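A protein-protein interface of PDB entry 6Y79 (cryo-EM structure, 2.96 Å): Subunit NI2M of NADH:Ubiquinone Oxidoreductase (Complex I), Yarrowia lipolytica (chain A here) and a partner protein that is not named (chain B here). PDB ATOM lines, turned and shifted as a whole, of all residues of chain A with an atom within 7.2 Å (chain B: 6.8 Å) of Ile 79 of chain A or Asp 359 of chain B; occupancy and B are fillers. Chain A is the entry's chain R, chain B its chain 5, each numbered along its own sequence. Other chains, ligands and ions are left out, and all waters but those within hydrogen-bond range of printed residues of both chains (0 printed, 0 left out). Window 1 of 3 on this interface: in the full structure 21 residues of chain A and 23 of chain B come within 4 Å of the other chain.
Along chain B the printed residues that touch a printed residue of chain A span positions 299 to 362. Hydrophobic or aromatic side chains of chain A within 4 Å of the printed part of chain B: His 75 and Ile 79. Along chain A the printed residues that touch a printed residue of chain B span positions 27 to 88. Among the printed residues, 10 pairs touch across the chains. Among the printed residues, no Asp or Glu carboxylate lies within 4 Å of a Lys or Arg side-chain nitrogen of the other chain.
The backbone carbonyl oxygen of Asn 28 of chain A is in hydrogen-bond range of a ring nitrogen (NE2) of His 75 of chain A (3.4 Å). The backbone carbonyl oxygen of Asp 77 of chain A lies within hydrogen-bond range of the side-chain amide nitrogen of Asn 28 of chain A (3.4 Å). O of Asn 299 of chain B lies close to N of Ile 360 of chain B (3.3 Å). ND2 of Asn 299 of chain B lies close to NH1 of Arg 361 of chain B, at 3.3 Å. The side-chain carboxylate (OD2) of Asp 300 of chain B sits close to the side-chain amide oxygen (OE1) of Gln 358 of chain B, 3.0 Å away. O of Gln 358 of chain B lies within hydrogen-bond range of N of Leu 301 of chain B, 3.2 Å away.
Of chain B, only Asp 359 (3.7 Å), Arg 361 (3.4 Å) and Thr 362 (3.7 Å) come within 4 Å of Ile 79 of chain A. Of chain A, only Ile 79 (3.7 Å) and Val 80 (3.9 Å) come within 4 Å of Asp 359 of chain B. Of the printed residues of chain B, Arg 27 of chain A touches Arg 361. Of the printed residues of chain B, His 75 of chain A touches Arg 361. Of the printed residues of chain B, Asn 28 of chain A touches Arg 361. Printed residues of chain A within 4 Å of Thr 362 of chain B: Ile 79. Pro 81 of chain A touches none of the printed residues of chain B. Ile 353 of chain B touches none of the printed residues of chain A. The nearest residue of chain B that does not touch Ile 79 of chain A is Ser 357 of chain B (6.0 Å). The nearest residue of chain A that does not touch Asp 359 of chain B is Pro 78 of chain A (4.4 Å). The nearest printed residue of chain B that does not touch His 75 of chain A is Asn 299 of chain B (4.5 Å).
OD1 of Asn 299 of chain B sits close to OD2 of Asp 77 of chain A (3.3 Å).
NH2 of Arg 27 of chain A touches O of Arg 361 of chain B, 3.6 Å away. Asn 28 of chain A touches Arg 361 of chain B. His 75 of chain A touches Arg 361 of chain B (CE1 to NH1, 3.3 Å). O of Asp 77 of chain A touches NH2 of Arg 361 of chain B, at 3.6 Å. OD2 of Asp 359 of chain B touches CA of Ile 79 of chain A, at 3.7 Å. Ile 79 of chain A touches Arg 361 of chain B (CG1 to NH2, 3.4 Å). Ile 79 of chain A touches Thr 362 of chain B. Asp 359 of chain B touches Val 80 of chain A. Thr 88 of chain A touches Gln 358 of chain B (CG2 to OE1, 3.4 Å).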
ATOM      1  N   LYS A  24       5.415  -8.923  -2.140  1.00  0.00           N
ATOM      2  CA  LYS A  24       4.751  -8.125  -3.169  1.00  0.00           C
ATOM      3  C   LYS A  24       5.574  -8.074  -4.441  1.00  0.00           C
ATOM      4  O   LYS A  24       5.027  -8.035  -5.548  1.00  0.00           O
ATOM      5  CB  LYS A  24       4.541  -6.701  -2.673  1.00  0.00           C
ATOM      6  CG  LYS A  24       3.328  -6.463  -1.845  1.00  0.00           C
ATOM      7  CD  LYS A  24       3.311  -4.993  -1.497  1.00  0.00           C
ATOM      8  CE  LYS A  24       2.518  -4.705  -0.254  1.00  0.00           C
ATOM      9  NZ  LYS A  24       2.437  -3.243  -0.046  1.00  0.00           N
ATOM     10  N   ARG A  27       5.387 -11.190  -6.301  1.00  0.00           N
ATOM     11  CA  ARG A  27       4.032 -11.396  -6.809  1.00  0.00           C
ATOM     12  C   ARG A  27       3.904 -11.053  -8.291  1.00  0.00           C
ATOM     13  O   ARG A  27       3.235 -11.775  -9.039  1.00  0.00           O
ATOM     14  CB  ARG A  27       3.045 -10.582  -5.973  1.00  0.00           C
ATOM     15  CG  ARG A  27       1.635 -10.506  -6.520  1.00  0.00           C
ATOM     16  CD  ARG A  27       0.970 -11.863  -6.536  1.00  0.00           C
ATOM     17  NE  ARG A  27      -0.302 -11.821  -7.244  1.00  0.00           N
ATOM     18  CZ  ARG A  27      -0.434 -12.013  -8.553  1.00  0.00           C
ATOM     19  NH1 ARG A  27       0.636 -12.263  -9.297  1.00  0.00           N
ATOM     20  NH2 ARG A  27      -1.633 -11.959  -9.116  1.00  0.00           N
ATOM     21  N   ASN A  28       4.554  -9.982  -8.750  1.00  0.00           N
ATOM     22  CA  ASN A  28       4.350  -9.566 -10.130  1.00  0.00           C
ATOM     23  C   ASN A  28       5.376 -10.122 -11.112  1.00  0.00           C
ATOM     24  O   ASN A  28       5.211  -9.927 -12.318  1.00  0.00           O
ATOM     25  CB  ASN A  28       4.285  -8.032 -10.232  1.00  0.00           C
ATOM     26  CG  ASN A  28       5.460  -7.332  -9.593  1.00  0.00           C
ATOM     27  OD1 ASN A  28       6.552  -7.872  -9.483  1.00  0.00           O
ATOM     28  ND2 ASN A  28       5.231  -6.103  -9.164  1.00  0.00           N
ATOM     29  N   TRP A  29       6.420 -10.807 -10.647  1.00  0.00           N
ATOM     30  CA  TRP A  29       7.262 -11.535 -11.593  1.00  0.00           C
ATOM     31  C   TRP A  29       6.559 -12.785 -12.105  1.00  0.00           C
ATOM     32  O   TRP A  29       6.519 -13.033 -13.311  1.00  0.00           O
ATOM     33  CB  TRP A  29       8.593 -11.935 -10.964  1.00  0.00           C
ATOM     34  CG  TRP A  29       9.546 -10.834 -10.663  1.00  0.00           C
ATOM     35  CD1 TRP A  29       9.825 -10.325  -9.442  1.00  0.00           C
ATOM     36  CD2 TRP A  29      10.394 -10.145 -11.585  1.00  0.00           C
ATOM     37  NE1 TRP A  29      10.765  -9.338  -9.534  1.00  0.00           N
ATOM     38  CE2 TRP A  29      11.137  -9.211 -10.844  1.00  0.00           C
ATOM     39  CE3 TRP A  29      10.589 -10.218 -12.965  1.00  0.00           C
ATOM     40  CZ2 TRP A  29      12.059  -8.360 -11.430  1.00  0.00           C
ATOM     41  CZ3 TRP A  29      11.504  -9.366 -13.549  1.00  0.00           C
ATOM     42  CH2 TRP A  29      12.228  -8.449 -12.782  1.00  0.00           C
ATOM     43  N   ILE A  30       5.989 -13.580 -11.211  1.00  0.00           N
ATOM     44  CA  ILE A  30       5.557 -14.931 -11.542  1.00  0.00           C
ATOM     45  C   ILE A  30       4.103 -14.906 -11.988  1.00  0.00           C
ATOM     46  O   ILE A  30       3.223 -14.426 -11.264  1.00  0.00           O
ATOM     47  CB  ILE A  30       5.765 -15.888 -10.361  1.00  0.00           C
ATOM     48  CG1 ILE A  30       7.255 -15.979 -10.040  1.00  0.00           C
ATOM     49  CG2 ILE A  30       5.244 -17.255 -10.716  1.00  0.00           C
ATOM     50  CD1 ILE A  30       7.559 -16.356  -8.622  1.00  0.00           C
ATOM     51  N   HIS A  75      10.605  -4.450 -10.175  1.00  0.00           N
ATOM     52  CA  HIS A  75       9.748  -4.656 -11.332  1.00  0.00           C
ATOM     53  C   HIS A  75       9.342  -3.326 -11.963  1.00  0.00           C
ATOM     54  O   HIS A  75       9.214  -2.317 -11.259  1.00  0.00           O
ATOM     55  CB  HIS A  75       8.494  -5.442 -10.925  1.00  0.00           C
ATOM     56  CG  HIS A  75       7.847  -6.172 -12.057  1.00  0.00           C
ATOM     57  ND1 HIS A  75       6.880  -5.599 -12.850  1.00  0.00           N
ATOM     58  CD2 HIS A  75       8.059  -7.409 -12.557  1.00  0.00           C
ATOM     59  CE1 HIS A  75       6.507  -6.460 -13.778  1.00  0.00           C
ATOM     60  NE2 HIS A  75       7.207  -7.567 -13.622  1.00  0.00           N
ATOM     61  N   ASP A  77       6.315  -2.577 -13.776  1.00  0.00           N
ATOM     62  CA  ASP A  77       4.932  -2.374 -13.382  1.00  0.00           C
ATOM     63  C   ASP A  77       4.698  -3.096 -12.070  1.00  0.00           C
ATOM     64  O   ASP A  77       4.783  -4.328 -12.045  1.00  0.00           O
ATOM     65  CB  ASP A  77       3.956  -2.933 -14.417  1.00  0.00           C
ATOM     66  CG  ASP A  77       3.968  -2.191 -15.718  1.00  0.00           C
ATOM     67  OD1 ASP A  77       4.235  -0.978 -15.710  1.00  0.00           O
ATOM     68  OD2 ASP A  77       3.708  -2.841 -16.749  1.00  0.00           O
ATOM     69  N   PRO A  78       4.416  -2.428 -10.969  1.00  0.00           N
ATOM     70  CA  PRO A  78       3.760  -3.127  -9.870  1.00  0.00           C
ATOM     71  C   PRO A  78       2.300  -3.378 -10.206  1.00  0.00           C
ATOM     72  O   PRO A  78       1.639  -2.583 -10.873  1.00  0.00           O
ATOM     73  CB  PRO A  78       3.919  -2.160  -8.696  1.00  0.00           C
ATOM     74  CG  PRO A  78       4.071  -0.830  -9.306  1.00  0.00           C
ATOM     75  CD  PRO A  78       4.793  -1.047 -10.607  1.00  0.00           C
ATOM     76  N   ILE A  79       1.809  -4.530  -9.768  1.00  0.00           N
ATOM     77  CA  ILE A  79       0.378  -4.807  -9.819  1.00  0.00           C
ATOM     78  C   ILE A  79      -0.287  -3.876  -8.817  1.00  0.00           C
ATOM     79  O   ILE A  79       0.071  -3.888  -7.642  1.00  0.00           O
ATOM     80  CB  ILE A  79       0.074  -6.274  -9.503  1.00  0.00           C
ATOM     81  CG1 ILE A  79       0.566  -7.171 -10.630  1.00  0.00           C
ATOM     82  CG2 ILE A  79      -1.406  -6.473  -9.303  1.00  0.00           C
ATOM     83  CD1 ILE A  79       0.435  -8.634 -10.334  1.00  0.00           C
ATOM     84  N   VAL A  80      -1.196  -3.022  -9.285  1.00  0.00           N
ATOM     85  CA  VAL A  80      -1.946  -2.082  -8.447  1.00  0.00           C
ATOM     86  C   VAL A  80      -3.424  -2.360  -8.687  1.00  0.00           C
ATOM     87  O   VAL A  80      -3.800  -2.708  -9.815  1.00  0.00           O
ATOM     88  CB  VAL A  80      -1.613  -0.615  -8.790  1.00  0.00           C
ATOM     89  CG1 VAL A  80      -2.081   0.356  -7.717  1.00  0.00           C
ATOM     90  CG2 VAL A  80      -0.129  -0.421  -9.030  1.00  0.00           C
ATOM     91  N   PRO A  81      -4.305  -2.241  -7.695  1.00  0.00           N
ATOM     92  CA  PRO A  81      -5.721  -2.229  -8.006  1.00  0.00           C
ATOM     93  C   PRO A  81      -6.091  -0.867  -8.554  1.00  0.00           C
ATOM     94  O   PRO A  81      -5.519   0.152  -8.134  1.00  0.00           O
ATOM     95  CB  PRO A  81      -6.397  -2.499  -6.651  1.00  0.00           C
ATOM     96  CG  PRO A  81      -5.305  -2.846  -5.725  1.00  0.00           C
ATOM     97  CD  PRO A  81      -4.116  -2.172  -6.242  1.00  0.00           C
ATOM     98  N   THR A  88      -5.634   2.531 -12.770  1.00  0.00           N
ATOM     99  CA  THR A  88      -6.298   3.096 -13.932  1.00  0.00           C
ATOM    100  C   THR A  88      -7.650   3.718 -13.620  1.00  0.00           C
ATOM    101  O   THR A  88      -8.108   4.569 -14.385  1.00  0.00           O
ATOM    102  CB  THR A  88      -6.487   2.010 -14.989  1.00  0.00           C
ATOM    103  OG1 THR A  88      -7.518   1.113 -14.562  1.00  0.00           O
ATOM    104  CG2 THR A  88      -5.211   1.229 -15.157  1.00  0.00           C
ATOM    105  N   ASN B 299       2.530  -5.854 -20.145  1.00  0.00           N
ATOM    106  CA  ASN B 299       1.603  -6.604 -19.303  1.00  0.00           C
ATOM    107  C   ASN B 299       0.191  -6.048 -19.237  1.00  0.00           C
ATOM    108  O   ASN B 299      -0.703  -6.785 -18.816  1.00  0.00           O
ATOM    109  CB  ASN B 299       2.145  -6.688 -17.873  1.00  0.00           C
ATOM    110  CG  ASN B 299       3.638  -6.895 -17.831  1.00  0.00           C
ATOM    111  OD1 ASN B 299       4.401  -5.940 -17.699  1.00  0.00           O
ATOM    112  ND2 ASN B 299       4.066  -8.148 -17.921  1.00  0.00           N
ATOM    113  N   ASP B 300      -0.047  -4.790 -19.598  1.00  0.00           N
ATOM    114  CA  ASP B 300      -1.394  -4.242 -19.624  1.00  0.00           C
ATOM    115  C   ASP B 300      -2.089  -4.656 -20.909  1.00  0.00           C
ATOM    116  O   ASP B 300      -1.478  -4.654 -21.974  1.00  0.00           O
ATOM    117  CB  ASP B 300      -1.343  -2.720 -19.531  1.00  0.00           C
ATOM    118  CG  ASP B 300      -2.690  -2.105 -19.238  1.00  0.00           C
ATOM    119  OD1 ASP B 300      -3.515  -1.965 -20.165  1.00  0.00           O
ATOM    120  OD2 ASP B 300      -2.917  -1.741 -18.069  1.00  0.00           O
ATOM    121  N   LEU B 301      -3.374  -4.989 -20.806  1.00  0.00           N
ATOM    122  CA  LEU B 301      -4.120  -5.496 -21.956  1.00  0.00           C
ATOM    123  C   LEU B 301      -4.289  -4.433 -23.036  1.00  0.00           C
ATOM    124  O   LEU B 301      -4.082  -4.700 -24.231  1.00  0.00           O
ATOM    125  CB  LEU B 301      -5.475  -5.991 -21.485  1.00  0.00           C
ATOM    126  CG  LEU B 301      -6.355  -6.641 -22.527  1.00  0.00           C
ATOM    127  CD1 LEU B 301      -5.779  -7.957 -23.014  1.00  0.00           C
ATOM    128  CD2 LEU B 301      -7.648  -6.830 -21.854  1.00  0.00           C
ATOM    129  N   ILE B 353     -15.056  -7.871 -15.122  1.00  0.00           N
ATOM    130  CA  ILE B 353     -14.407  -8.055 -13.831  1.00  0.00           C
ATOM    131  C   ILE B 353     -14.884  -6.976 -12.866  1.00  0.00           C
ATOM    132  O   ILE B 353     -14.917  -5.788 -13.211  1.00  0.00           O
ATOM    133  CB  ILE B 353     -12.881  -8.045 -14.016  1.00  0.00           C
ATOM    134  CG1 ILE B 353     -12.455  -9.289 -14.788  1.00  0.00           C
ATOM    135  CG2 ILE B 353     -12.152  -7.986 -12.706  1.00  0.00           C
ATOM    136  CD1 ILE B 353     -10.984  -9.332 -15.092  1.00  0.00           C
ATOM    137  N   GLU B 356     -12.291  -4.260 -12.135  1.00  0.00           N
ATOM    138  CA  GLU B 356     -11.951  -3.397 -13.280  1.00  0.00           C
ATOM    139  C   GLU B 356     -10.427  -3.296 -13.425  1.00  0.00           C
ATOM    140  O   GLU B 356      -9.838  -2.236 -13.632  1.00  0.00           O
ATOM    141  CB  GLU B 356     -12.647  -2.031 -13.171  1.00  0.00           C
ATOM    142  CG  GLU B 356     -12.625  -1.062 -14.340  1.00  0.00           C
ATOM    143  CD  GLU B 356     -13.278   0.240 -13.938  1.00  0.00           C
ATOM    144  OE1 GLU B 356     -13.971   0.245 -12.901  1.00  0.00           O
ATOM    145  OE2 GLU B 356     -12.984   1.272 -14.563  1.00  0.00           O
ATOM    146  N   SER B 357      -9.772  -4.438 -13.319  1.00  0.00           N
ATOM    147  CA  SER B 357      -8.333  -4.418 -13.491  1.00  0.00           C
ATOM    148  C   SER B 357      -7.972  -4.544 -14.964  1.00  0.00           C
ATOM    149  O   SER B 357      -8.775  -4.953 -15.805  1.00  0.00           O
ATOM    150  CB  SER B 357      -7.667  -5.528 -12.683  1.00  0.00           C
ATOM    151  OG  SER B 357      -6.300  -5.212 -12.505  1.00  0.00           O
ATOM    152  N   GLN B 358      -6.734  -4.184 -15.264  1.00  0.00           N
ATOM    153  CA  GLN B 358      -6.197  -4.266 -16.605  1.00  0.00           C
ATOM    154  C   GLN B 358      -4.947  -5.117 -16.698  1.00  0.00           C
ATOM    155  O   GLN B 358      -4.534  -5.440 -17.816  1.00  0.00           O
ATOM    156  CB  GLN B 358      -5.880  -2.866 -17.143  1.00  0.00           C
ATOM    157  CG  GLN B 358      -7.091  -2.037 -17.460  1.00  0.00           C
ATOM    158  CD  GLN B 358      -6.724  -0.684 -18.020  1.00  0.00           C
ATOM    159  OE1 GLN B 358      -5.548  -0.362 -18.181  1.00  0.00           O
ATOM    160  NE2 GLN B 358      -7.729   0.120 -18.317  1.00  0.00           N
ATOM    161  N   ASP B 359      -4.323  -5.475 -15.578  1.00  0.00           N
ATOM    162  CA  ASP B 359      -3.150  -6.332 -15.641  1.00  0.00           C
ATOM    163  C   ASP B 359      -3.599  -7.746 -15.961  1.00  0.00           C
ATOM    164  O   ASP B 359      -4.483  -8.288 -15.286  1.00  0.00           O
ATOM    165  CB  ASP B 359      -2.388  -6.306 -14.328  1.00  0.00           C
ATOM    166  CG  ASP B 359      -1.771  -4.957 -14.033  1.00  0.00           C
ATOM    167  OD1 ASP B 359      -1.343  -4.243 -14.963  1.00  0.00           O
ATOM    168  OD2 ASP B 359      -1.743  -4.597 -12.836  1.00  0.00           O
ATOM    169  N   ILE B 360      -3.003  -8.341 -17.000  1.00  0.00           N
ATOM    170  CA  ILE B 360      -3.390  -9.691 -17.399  1.00  0.00           C
ATOM    171  C   ILE B 360      -2.823 -10.722 -16.443  1.00  0.00           C
ATOM    172  O   ILE B 360      -3.270 -11.872 -16.423  1.00  0.00           O
ATOM    173  CB  ILE B 360      -2.958  -9.973 -18.847  1.00  0.00           C
ATOM    174  CG1 ILE B 360      -1.430 -10.002 -18.951  1.00  0.00           C
ATOM    175  CG2 ILE B 360      -3.559  -8.957 -19.800  1.00  0.00           C
ATOM    176  CD1 ILE B 360      -0.931 -10.222 -20.343  1.00  0.00           C
ATOM    177  N   ARG B 361      -1.845 -10.327 -15.624  1.00  0.00           N
ATOM    178  CA  ARG B 361      -1.387 -11.143 -14.508  1.00  0.00           C
ATOM    179  C   ARG B 361      -2.466 -11.333 -13.452  1.00  0.00           C
ATOM    180  O   ARG B 361      -2.338 -12.219 -12.601  1.00  0.00           O
ATOM    181  CB  ARG B 361      -0.165 -10.489 -13.870  1.00  0.00           C
ATOM    182  CG  ARG B 361       1.082 -10.484 -14.724  1.00  0.00           C
ATOM    183  CD  ARG B 361       2.218  -9.883 -13.926  1.00  0.00           C
ATOM    184  NE  ARG B 361       1.873  -8.535 -13.487  1.00  0.00           N
ATOM    185  CZ  ARG B 361       2.490  -7.438 -13.902  1.00  0.00           C
ATOM    186  NH1 ARG B 361       3.504  -7.537 -14.738  1.00  0.00           N
ATOM    187  NH2 ARG B 361       2.113  -6.248 -13.469  1.00  0.00           N
ATOM    188  N   THR B 362      -3.509 -10.509 -13.469  1.00  0.00           N
ATOM    189  CA  THR B 362      -4.576 -10.566 -12.485  1.00  0.00           C
ATOM    190  C   THR B 362      -5.873 -11.097 -13.072  1.00  0.00           C
ATOM    191  O   THR B 362      -6.909 -11.057 -12.407  1.00  0.00           O
ATOM    192  CB  THR B 362      -4.813  -9.178 -11.903  1.00  0.00           C
ATOM    193  OG1 THR B 362      -5.435  -8.366 -12.908  1.00  0.00           O
ATOM    194  CG2 THR B 362      -3.515  -8.550 -11.497  1.00  0.00           C
ATOM    195  N   TYR B 363      -5.849 -11.584 -14.308  1.00  0.00           N
ATOM    196  CA  TYR B 363      -7.095 -12.016 -14.924  1.00  0.00           C
ATOM    197  C   TYR B 363      -7.415 -13.450 -14.545  1.00  0.00           C
ATOM    198  O   TYR B 363      -8.481 -13.732 -13.992  1.00  0.00           O
ATOM    199  CB  TYR B 363      -7.026 -11.883 -16.441  1.00  0.00           C
ATOM    200  CG  TYR B 363      -7.143 -10.474 -16.964  1.00  0.00           C
ATOM    201  CD1 TYR B 363      -7.464  -9.409 -16.127  1.00  0.00           C
ATOM    202  CD2 TYR B 363      -6.941 -10.209 -18.306  1.00  0.00           C
ATOM    203  CE1 TYR B 363      -7.569  -8.124 -16.622  1.00  0.00           C
ATOM    204  CE2 TYR B 363      -7.046  -8.936 -18.805  1.00  0.00           C
ATOM    205  CZ  TYR B 363      -7.357  -7.899 -17.966  1.00  0.00           C
ATOM    206  OH  TYR B 363      -7.454  -6.635 -18.495  1.00  0.00           O
ATOM    207  N   GLY B 364      -6.503 -14.364 -14.831  1.00  0.00           N
ATOM    208  CA  GLY B 364      -6.771 -15.768 -14.624  1.00  0.00           C
ATOM    209  C   GLY B 364      -7.696 -16.306 -15.688  1.00  0.00           C
ATOM    210  O   GLY B 364      -8.038 -15.634 -16.641  1.00  0.00           O
